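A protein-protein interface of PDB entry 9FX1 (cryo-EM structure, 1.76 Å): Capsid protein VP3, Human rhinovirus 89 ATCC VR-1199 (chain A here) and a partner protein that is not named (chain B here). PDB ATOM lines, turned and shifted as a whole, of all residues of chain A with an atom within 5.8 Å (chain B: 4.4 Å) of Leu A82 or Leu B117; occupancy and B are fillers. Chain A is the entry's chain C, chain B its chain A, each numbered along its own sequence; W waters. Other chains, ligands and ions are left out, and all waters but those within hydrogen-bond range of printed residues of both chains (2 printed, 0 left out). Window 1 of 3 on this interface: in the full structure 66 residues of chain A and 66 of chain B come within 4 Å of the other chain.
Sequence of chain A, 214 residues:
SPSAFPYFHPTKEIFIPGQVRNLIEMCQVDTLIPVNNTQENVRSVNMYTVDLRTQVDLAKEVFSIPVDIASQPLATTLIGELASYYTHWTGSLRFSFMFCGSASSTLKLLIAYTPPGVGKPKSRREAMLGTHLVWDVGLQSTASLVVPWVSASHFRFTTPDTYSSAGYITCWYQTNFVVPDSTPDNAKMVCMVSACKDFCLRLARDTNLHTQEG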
ATOM      1  N   LEU A  23      27.079   9.121  18.005  1.00  0.00           N
ATOM      2  CA  LEU A  23      27.653  10.456  18.240  1.00  0.00           C
ATOM      3  C   LEU A  23      28.422  10.553  19.561  1.00  0.00           C
ATOM      4  O   LEU A  23      29.278  11.423  19.702  1.00  0.00           O
ATOM      5  CB  LEU A  23      26.558  11.531  18.247  1.00  0.00           C
ATOM      6  CG  LEU A  23      25.858  11.803  16.912  1.00  0.00           C
ATOM      7  CD1 LEU A  23      24.816  12.886  17.172  1.00  0.00           C
ATOM      8  CD2 LEU A  23      26.826  12.282  15.837  1.00  0.00           C
ATOM      9  N   MET A  26      32.138  10.506  19.184  1.00  0.00           N
ATOM     10  CA  MET A  26      32.677  11.824  18.848  1.00  0.00           C
ATOM     11  C   MET A  26      32.744  12.742  20.083  1.00  0.00           C
ATOM     12  O   MET A  26      33.729  13.449  20.269  1.00  0.00           O
ATOM     13  CB  MET A  26      31.819  12.447  17.734  1.00  0.00           C
ATOM     14  CG  MET A  26      31.843  11.621  16.444  1.00  0.00           C
ATOM     15  SD  MET A  26      30.518  12.011  15.279  1.00  0.00           S
ATOM     16  CE  MET A  26      30.846  13.744  14.874  1.00  0.00           C
ATOM     17  N   CYS A  27      31.748  12.703  20.975  1.00  0.00           N
ATOM     18  CA  CYS A  27      31.777  13.458  22.243  1.00  0.00           C
ATOM     19  C   CYS A  27      32.918  13.009  23.173  1.00  0.00           C
ATOM     20  O   CYS A  27      33.412  13.782  23.989  1.00  0.00           O
ATOM     21  CB  CYS A  27      30.444  13.278  22.983  1.00  0.00           C
ATOM     22  SG  CYS A  27      29.053  13.936  22.020  1.00  0.00           S
ATOM     23  N   THR A  77      32.571  23.795  20.916  1.00  0.00           N
ATOM     24  CA  THR A  77      33.327  22.534  20.997  1.00  0.00           C
ATOM     25  C   THR A  77      32.530  21.404  20.357  1.00  0.00           C
ATOM     26  O   THR A  77      31.320  21.518  20.206  1.00  0.00           O
ATOM     27  CB  THR A  77      33.655  22.132  22.437  1.00  0.00           C
ATOM     28  OG1 THR A  77      32.492  21.787  23.150  1.00  0.00           O
ATOM     29  CG2 THR A  77      34.387  23.248  23.175  1.00  0.00           C
ATOM     30  N   LEU A  78      33.163  20.296  19.980  1.00  0.00           N
ATOM     31  CA  LEU A  78      32.427  19.212  19.333  1.00  0.00           C
ATOM     32  C   LEU A  78      31.347  18.638  20.257  1.00  0.00           C
ATOM     33  O   LEU A  78      30.203  18.496  19.839  1.00  0.00           O
ATOM     34  CB  LEU A  78      33.409  18.145  18.842  1.00  0.00           C
ATOM     35  CG  LEU A  78      32.746  16.988  18.082  1.00  0.00           C
ATOM     36  CD1 LEU A  78      32.055  17.466  16.804  1.00  0.00           C
ATOM     37  CD2 LEU A  78      33.845  16.014  17.676  1.00  0.00           C
ATOM     38  N   ILE A  79      31.667  18.379  21.525  1.00  0.00           N
ATOM     39  CA  ILE A  79      30.662  17.943  22.500  1.00  0.00           C
ATOM     40  C   ILE A  79      29.551  18.988  22.683  1.00  0.00           C
ATOM     41  O   ILE A  79      28.387  18.610  22.718  1.00  0.00           O
ATOM     42  CB  ILE A  79      31.322  17.540  23.832  1.00  0.00           C
ATOM     43  CG1 ILE A  79      30.286  16.896  24.774  1.00  0.00           C
ATOM     44  CG2 ILE A  79      32.014  18.728  24.520  1.00  0.00           C
ATOM     45  CD1 ILE A  79      30.931  16.207  25.981  1.00  0.00           C
ATOM     46  N   GLY A  80      29.855  20.287  22.728  1.00  0.00           N
ATOM     47  CA  GLY A  80      28.831  21.334  22.829  1.00  0.00           C
ATOM     48  C   GLY A  80      27.951  21.422  21.577  1.00  0.00           C
ATOM     49  O   GLY A  80      26.727  21.539  21.655  1.00  0.00           O
ATOM     50  N   GLU A  81      28.550  21.263  20.404  1.00  0.00           N
ATOM     51  CA  GLU A  81      27.841  21.265  19.133  1.00  0.00           C
ATOM     52  C   GLU A  81      26.908  20.068  19.009  1.00  0.00           C
ATOM     53  O   GLU A  81      25.743  20.243  18.669  1.00  0.00           O
ATOM     54  CB  GLU A  81      28.849  21.240  17.982  1.00  0.00           C
ATOM     55  CG  GLU A  81      29.570  22.579  17.814  1.00  0.00           C
ATOM     56  CD  GLU A  81      28.740  23.626  17.073  1.00  0.00           C
ATOM     57  OE1 GLU A  81      27.535  23.400  16.804  1.00  0.00           O
ATOM     58  OE2 GLU A  81      29.328  24.657  16.670  1.00  0.00           O
ATOM     59  N   LEU A  82      27.387  18.867  19.327  1.00  0.00           N
ATOM     60  CA  LEU A  82      26.564  17.662  19.327  1.00  0.00           C
ATOM     61  C   LEU A  82      25.494  17.738  20.412  1.00  0.00           C
ATOM     62  O   LEU A  82      24.333  17.486  20.125  1.00  0.00           O
ATOM     63  CB  LEU A  82      27.454  16.418  19.470  1.00  0.00           C
ATOM     64  CG  LEU A  82      28.421  16.228  18.288  1.00  0.00           C
ATOM     65  CD1 LEU A  82      29.328  15.033  18.558  1.00  0.00           C
ATOM     66  CD2 LEU A  82      27.683  16.001  16.967  1.00  0.00           C
ATOM     67  N   ALA A  83      25.828  18.206  21.616  1.00  0.00           N
ATOM     68  CA  ALA A  83      24.837  18.413  22.663  1.00  0.00           C
ATOM     69  C   ALA A  83      23.725  19.370  22.227  1.00  0.00           C
ATOM     70  O   ALA A  83      22.565  19.144  22.545  1.00  0.00           O
ATOM     71  CB  ALA A  83      25.526  18.944  23.913  1.00  0.00           C
ATOM     72  N   SER A  84      24.040  20.407  21.454  1.00  0.00           N
ATOM     73  CA  SER A  84      23.024  21.343  20.968  1.00  0.00           C
ATOM     74  C   SER A  84      22.090  20.761  19.887  1.00  0.00           C
ATOM     75  O   SER A  84      21.089  21.387  19.575  1.00  0.00           O
ATOM     76  CB  SER A  84      23.681  22.644  20.522  1.00  0.00           C
ATOM     77  OG  SER A  84      24.386  22.443  19.334  1.00  0.00           O
ATOM     78  N   TYR A  85      22.339  19.557  19.365  1.00  0.00           N
ATOM     79  CA  TYR A  85      21.337  18.778  18.616  1.00  0.00           C
ATOM     80  C   TYR A  85      20.384  17.980  19.515  1.00  0.00           C
ATOM     81  O   TYR A  85      19.541  17.236  19.027  1.00  0.00           O
ATOM     82  CB  TYR A  85      22.028  17.835  17.623  1.00  0.00           C
ATOM     83  CG  TYR A  85      22.473  18.542  16.372  1.00  0.00           C
ATOM     84  CD1 TYR A  85      21.492  18.981  15.462  1.00  0.00           C
ATOM     85  CD2 TYR A  85      23.837  18.741  16.098  1.00  0.00           C
ATOM     86  CE1 TYR A  85      21.873  19.629  14.276  1.00  0.00           C
ATOM     87  CE2 TYR A  85      24.222  19.369  14.902  1.00  0.00           C
ATOM     88  CZ  TYR A  85      23.243  19.825  13.995  1.00  0.00           C
ATOM     89  OH  TYR A  85      23.624  20.486  12.869  1.00  0.00           O
ATOM     90  N   TYR A  86      20.499  18.115  20.830  1.00  0.00           N
ATOM     91  CA  TYR A  86      19.721  17.358  21.801  1.00  0.00           C
ATOM     92  C   TYR A  86      19.225  18.271  22.917  1.00  0.00           C
ATOM     93  O   TYR A  86      19.778  19.335  23.173  1.00  0.00           O
ATOM     94  CB  TYR A  86      20.563  16.194  22.322  1.00  0.00           C
ATOM     95  CG  TYR A  86      20.768  15.107  21.281  1.00  0.00           C
ATOM     96  CD1 TYR A  86      21.840  15.162  20.376  1.00  0.00           C
ATOM     97  CD2 TYR A  86      19.850  14.049  21.196  1.00  0.00           C
ATOM     98  CE1 TYR A  86      21.975  14.179  19.376  1.00  0.00           C
ATOM     99  CE2 TYR A  86      19.994  13.043  20.226  1.00  0.00           C
ATOM    100  CZ  TYR A  86      21.054  13.113  19.302  1.00  0.00           C
ATOM    101  OH  TYR A  86      21.188  12.158  18.348  1.00  0.00           O
ATOM    102  N   LEU A 201      23.132  11.869  25.652  1.00  0.00           N
ATOM    103  CA  LEU A 201      22.214  12.877  25.129  1.00  0.00           C
ATOM    104  C   LEU A 201      20.891  12.187  24.768  1.00  0.00           C
ATOM    105  O   LEU A 201      20.891  11.028  24.352  1.00  0.00           O
ATOM    106  CB  LEU A 201      22.830  13.552  23.893  1.00  0.00           C
ATOM    107  CG  LEU A 201      24.195  14.228  24.094  1.00  0.00           C
ATOM    108  CD1 LEU A 201      24.793  14.603  22.737  1.00  0.00           C
ATOM    109  CD2 LEU A 201      24.043  15.486  24.941  1.00  0.00           C
ATOM    110  N   PHE B  70      20.190   9.752  14.603  1.00  0.00           N
ATOM    111  CA  PHE B  70      20.575  11.136  14.349  1.00  0.00           C
ATOM    112  C   PHE B  70      20.262  11.588  12.916  1.00  0.00           C
ATOM    113  O   PHE B  70      19.676  12.652  12.725  1.00  0.00           O
ATOM    114  CB  PHE B  70      22.061  11.299  14.675  1.00  0.00           C
ATOM    115  CG  PHE B  70      22.578  12.689  14.389  1.00  0.00           C
ATOM    116  CD1 PHE B  70      22.095  13.784  15.128  1.00  0.00           C
ATOM    117  CD2 PHE B  70      23.559  12.889  13.400  1.00  0.00           C
ATOM    118  CE1 PHE B  70      22.609  15.070  14.894  1.00  0.00           C
ATOM    119  CE2 PHE B  70      24.060  14.173  13.160  1.00  0.00           C
ATOM    120  CZ  PHE B  70      23.597  15.264  13.917  1.00  0.00           C
ATOM    121  N   ARG B 113      24.172  20.321   7.294  1.00  0.00           N
ATOM    122  CA  ARG B 113      25.115  20.377   8.417  1.00  0.00           C
ATOM    123  C   ARG B 113      25.243  19.048   9.154  1.00  0.00           C
ATOM    124  O   ARG B 113      26.356  18.657   9.496  1.00  0.00           O
ATOM    125  CB  ARG B 113      24.693  21.519   9.339  1.00  0.00           C
ATOM    126  CG  ARG B 113      25.760  21.773  10.407  1.00  0.00           C
ATOM    127  CD  ARG B 113      25.430  23.085  11.101  1.00  0.00           C
ATOM    128  NE  ARG B 113      26.464  23.468  12.075  1.00  0.00           N
ATOM    129  CZ  ARG B 113      26.464  23.224  13.365  1.00  0.00           C
ATOM    130  NH1 ARG B 113      27.306  23.856  14.119  1.00  0.00           N
ATOM    131  NH2 ARG B 113      25.644  22.377  13.909  1.00  0.00           N
ATOM    132  N   LYS B 114      24.127  18.338   9.341  1.00  0.00           N
ATOM    133  CA  LYS B 114      24.102  17.032  10.015  1.00  0.00           C
ATOM    134  C   LYS B 114      24.870  15.982   9.220  1.00  0.00           C
ATOM    135  O   LYS B 114      25.726  15.312   9.775  1.00  0.00           O
ATOM    136  CB  LYS B 114      22.655  16.580  10.267  1.00  0.00           C
ATOM    137  CG  LYS B 114      21.961  17.469  11.309  1.00  0.00           C
ATOM    138  CD  LYS B 114      20.481  17.109  11.496  1.00  0.00           C
ATOM    139  CE  LYS B 114      20.316  15.689  12.047  1.00  0.00           C
ATOM    140  NZ  LYS B 114      18.885  15.354  12.280  1.00  0.00           N
ATOM    141  N   TYR B 115      24.612  15.857   7.921  1.00  0.00           N
ATOM    142  CA  TYR B 115      25.314  14.861   7.101  1.00  0.00           C
ATOM    143  C   TYR B 115      26.796  15.230   6.946  1.00  0.00           C
ATOM    144  O   TYR B 115      27.665  14.370   6.978  1.00  0.00           O
ATOM    145  CB  TYR B 115      24.620  14.695   5.745  1.00  0.00           C
ATOM    146  CG  TYR B 115      23.304  13.940   5.808  1.00  0.00           C
ATOM    147  CD1 TYR B 115      22.193  14.493   6.466  1.00  0.00           C
ATOM    148  CD2 TYR B 115      23.184  12.667   5.214  1.00  0.00           C
ATOM    149  CE1 TYR B 115      20.971  13.807   6.527  1.00  0.00           C
ATOM    150  CE2 TYR B 115      21.953  11.981   5.255  1.00  0.00           C
ATOM    151  CZ  TYR B 115      20.841  12.557   5.901  1.00  0.00           C
ATOM    152  OH  TYR B 115      19.643  11.917   5.949  1.00  0.00           O
ATOM    153  N   GLU B 116      27.116  16.520   6.870  1.00  0.00           N
ATOM    154  CA  GLU B 116      28.496  17.003   6.824  1.00  0.00           C
ATOM    155  C   GLU B 116      29.294  16.861   8.132  1.00  0.00           C
ATOM    156  O   GLU B 116      30.484  17.165   8.146  1.00  0.00           O
ATOM    157  CB  GLU B 116      28.504  18.456   6.369  1.00  0.00           C
ATOM    158  CG  GLU B 116      28.263  18.578   4.859  1.00  0.00           C
ATOM    159  CD  GLU B 116      28.447  20.021   4.377  1.00  0.00           C
ATOM    160  OE1 GLU B 116      28.851  20.881   5.196  1.00  0.00           O
ATOM    161  OE2 GLU B 116      28.165  20.299   3.193  1.00  0.00           O
ATOM    162  N   LEU B 117      28.713  16.357   9.223  1.00  0.00           N
ATOM    163  CA  LEU B 117      29.514  15.852  10.348  1.00  0.00           C
ATOM    164  C   LEU B 117      30.355  14.625   9.972  1.00  0.00           C
ATOM    165  O   LEU B 117      31.201  14.211  10.753  1.00  0.00           O
ATOM    166  CB  LEU B 117      28.601  15.513  11.537  1.00  0.00           C
ATOM    167  CG  LEU B 117      28.181  16.750  12.343  1.00  0.00           C
ATOM    168  CD1 LEU B 117      27.005  16.393  13.244  1.00  0.00           C
ATOM    169  CD2 LEU B 117      29.339  17.238  13.219  1.00  0.00           C
ATOM    170  N   PHE B 118      30.153  14.050   8.788  1.00  0.00           N
ATOM    171  CA  PHE B 118      30.840  12.860   8.307  1.00  0.00           C
ATOM    172  C   PHE B 118      31.471  13.130   6.949  1.00  0.00           C
ATOM    173  O   PHE B 118      31.008  13.974   6.188  1.00  0.00           O
ATOM    174  CB  PHE B 118      29.863  11.687   8.263  1.00  0.00           C
ATOM    175  CG  PHE B 118      29.084  11.572   9.556  1.00  0.00           C
ATOM    176  CD1 PHE B 118      29.707  11.064  10.712  1.00  0.00           C
ATOM    177  CD2 PHE B 118      27.782  12.093   9.625  1.00  0.00           C
ATOM    178  CE1 PHE B 118      29.020  11.088  11.939  1.00  0.00           C
ATOM    179  CE2 PHE B 118      27.101  12.123  10.851  1.00  0.00           C
ATOM    180  CZ  PHE B 118      27.727  11.631  12.007  1.00  0.00           C
ATOM    181  N   CYS B 252      34.494   8.755   9.160  1.00  0.00           N
ATOM    182  CA  CYS B 252      35.450   9.849   9.287  1.00  0.00           C
ATOM    183  C   CYS B 252      34.750  11.130   9.749  1.00  0.00           C
ATOM    184  O   CYS B 252      34.413  11.987   8.922  1.00  0.00           O
ATOM    185  CB  CYS B 252      36.233  10.006   7.980  1.00  0.00           C
ATOM    186  SG  CYS B 252      37.027   8.440   7.542  1.00  0.00           S
ATOM    187  N   PRO B 253      34.498  11.256  11.059  1.00  0.00           N
ATOM    188  CA  PRO B 253      33.781  12.391  11.608  1.00  0.00           C
ATOM    189  C   PRO B 253      34.573  13.675  11.399  1.00  0.00           C
ATOM    190  O   PRO B 253      35.801  13.671  11.354  1.00  0.00           O
ATOM    191  CB  PRO B 253      33.559  12.084  13.086  1.00  0.00           C
ATOM    192  CG  PRO B 253      34.643  11.067  13.435  1.00  0.00           C
ATOM    193  CD  PRO B 253      34.921  10.347  12.115  1.00  0.00           C
ATOM    194  N   ARG B 254      33.862  14.786  11.289  1.00  0.00           N
ATOM    195  CA  ARG B 254      34.403  16.096  10.943  1.00  0.00           C
ATOM    196  C   ARG B 254      33.913  17.137  11.941  1.00  0.00           C
ATOM    197  O   ARG B 254      32.819  16.988  12.478  1.00  0.00           O
ATOM    198  CB  ARG B 254      33.947  16.509   9.540  1.00  0.00           C
ATOM    199  CG  ARG B 254      34.267  15.446   8.487  1.00  0.00           C
ATOM    200  CD  ARG B 254      33.864  15.962   7.112  1.00  0.00           C
ATOM    201  NE  ARG B 254      34.812  16.957   6.580  1.00  0.00           N
ATOM    202  CZ  ARG B 254      35.887  16.698   5.860  1.00  0.00           C
ATOM    203  NH1 ARG B 254      36.509  17.652   5.234  1.00  0.00           N
ATOM    204  NH2 ARG B 254      36.350  15.490   5.710  1.00  0.00           N
ATOM    205  N   PRO B 256      31.805  20.274  12.900  1.00  0.00           N
ATOM    206  CA  PRO B 256      30.590  20.809  12.304  1.00  0.00           C
ATOM    207  C   PRO B 256      30.863  22.147  11.621  1.00  0.00           C
ATOM    208  O   PRO B 256      31.741  22.909  12.036  1.00  0.00           O
ATOM    209  CB  PRO B 256      29.596  20.982  13.449  1.00  0.00           C
ATOM    210  CG  PRO B 256      30.485  21.092  14.681  1.00  0.00           C
ATOM    211  CD  PRO B 256      31.716  20.261  14.345  1.00  0.00           C
HETATM  212  O   HOH W   1      25.270  22.114  16.686  1.00  0.00           O
HETATM  213  O   HOH W   2      28.438  26.684  15.367  1.00  0.00           O
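The backbone carbonyl oxygen (O) of Leu A23 sits at hydrogen-bond distance from the side-chain sulfur (SG) of Cys A27.
The backbone NH (N) of Arg B254 sits at hydrogen-bond distance from the backbone carbonyl oxygen (O) of Leu B117, at 2.8 Å.
The side-chain hydroxyl (OG) of Ser A84 sits at hydrogen-bond distance from the backbone carbonyl oxygen (O) of Glu A81, at 2.7 Å.
The backbone carbonyl oxygen (O) of Phe B70 sits at hydrogen-bond distance from the side-chain amino group (NZ) of Lys B114.
Of the 14 printed residues of chain A, 7 touch a printed residue of chain B.
Of the 11 printed residues of chain B, 7 touch a printed residue of chain A.
Hydrophobic or aromatic side chains of chain B that line the printed part of chain A: Phe B70, Leu B117, Phe B118, Pro B253 and Pro B256.
Among the printed residues, Asp or Glu carboxylates within 4 Å of a Lys or Arg side-chain nitrogen of the other chain: Glu A81 with Arg B113 (2.7 Å).
The side-chain carboxylate (OE1) of Glu A81 is in salt-bridge range of the guanidinium group (NH1) of Arg B113 (2.7 Å).
OH of Tyr A85 is in hydrogen-bond range of NH2 of Arg B113, 3.0 Å away.
Of the printed residues of chain B, Glu A81 touches Arg B113 (2.7 Å) and Pro B256 (3.6 Å).
Leu A82 touches one residue of chain B.
Of the printed residues of chain A, Arg B113 touches Glu A81 and Tyr A85.
Leu B117 touches one residue of chain A.
The nearest printed residue of chain B that does not touch Leu A82 is Phe B70 (5.2 Å).
The nearest residue of chain A that does not touch Leu B117 is Met A26 (4.1 Å).
The nearest printed residue of chain A that does not touch Phe B70 is Leu A82 (5.2 Å).
Among the printed residues, merely in contact across the chains: Leu A23 with Phe B70 (3.5 Å), Leu A23 with Phe B118 (3.99 Å), Met A26 with Phe B118 (3.8 Å), Met A26 with Pro B253 (3.6 Å), Leu A78 with Pro B256 (3.7 Å), Glu A81 with Pro B256 (3.6 Å), Leu A82 with Leu B117 (3.8 Å), Tyr A85 with Phe B70 (3.8 Å), Tyr A85 with Lys B114 (3.7 Å) and Tyr A86 with Phe B70 (3.7 Å).
Water W2 bridges OE2 of Glu A81 and NH1 of Arg B113.
Water W1 lies within hydrogen-bond range of the side-chain carboxylate of Glu A81 (2.6 Å), the side-chain hydroxyl of Ser A84 (2.8 Å) and the guanidinium group of Arg B113 (2.8 Å).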
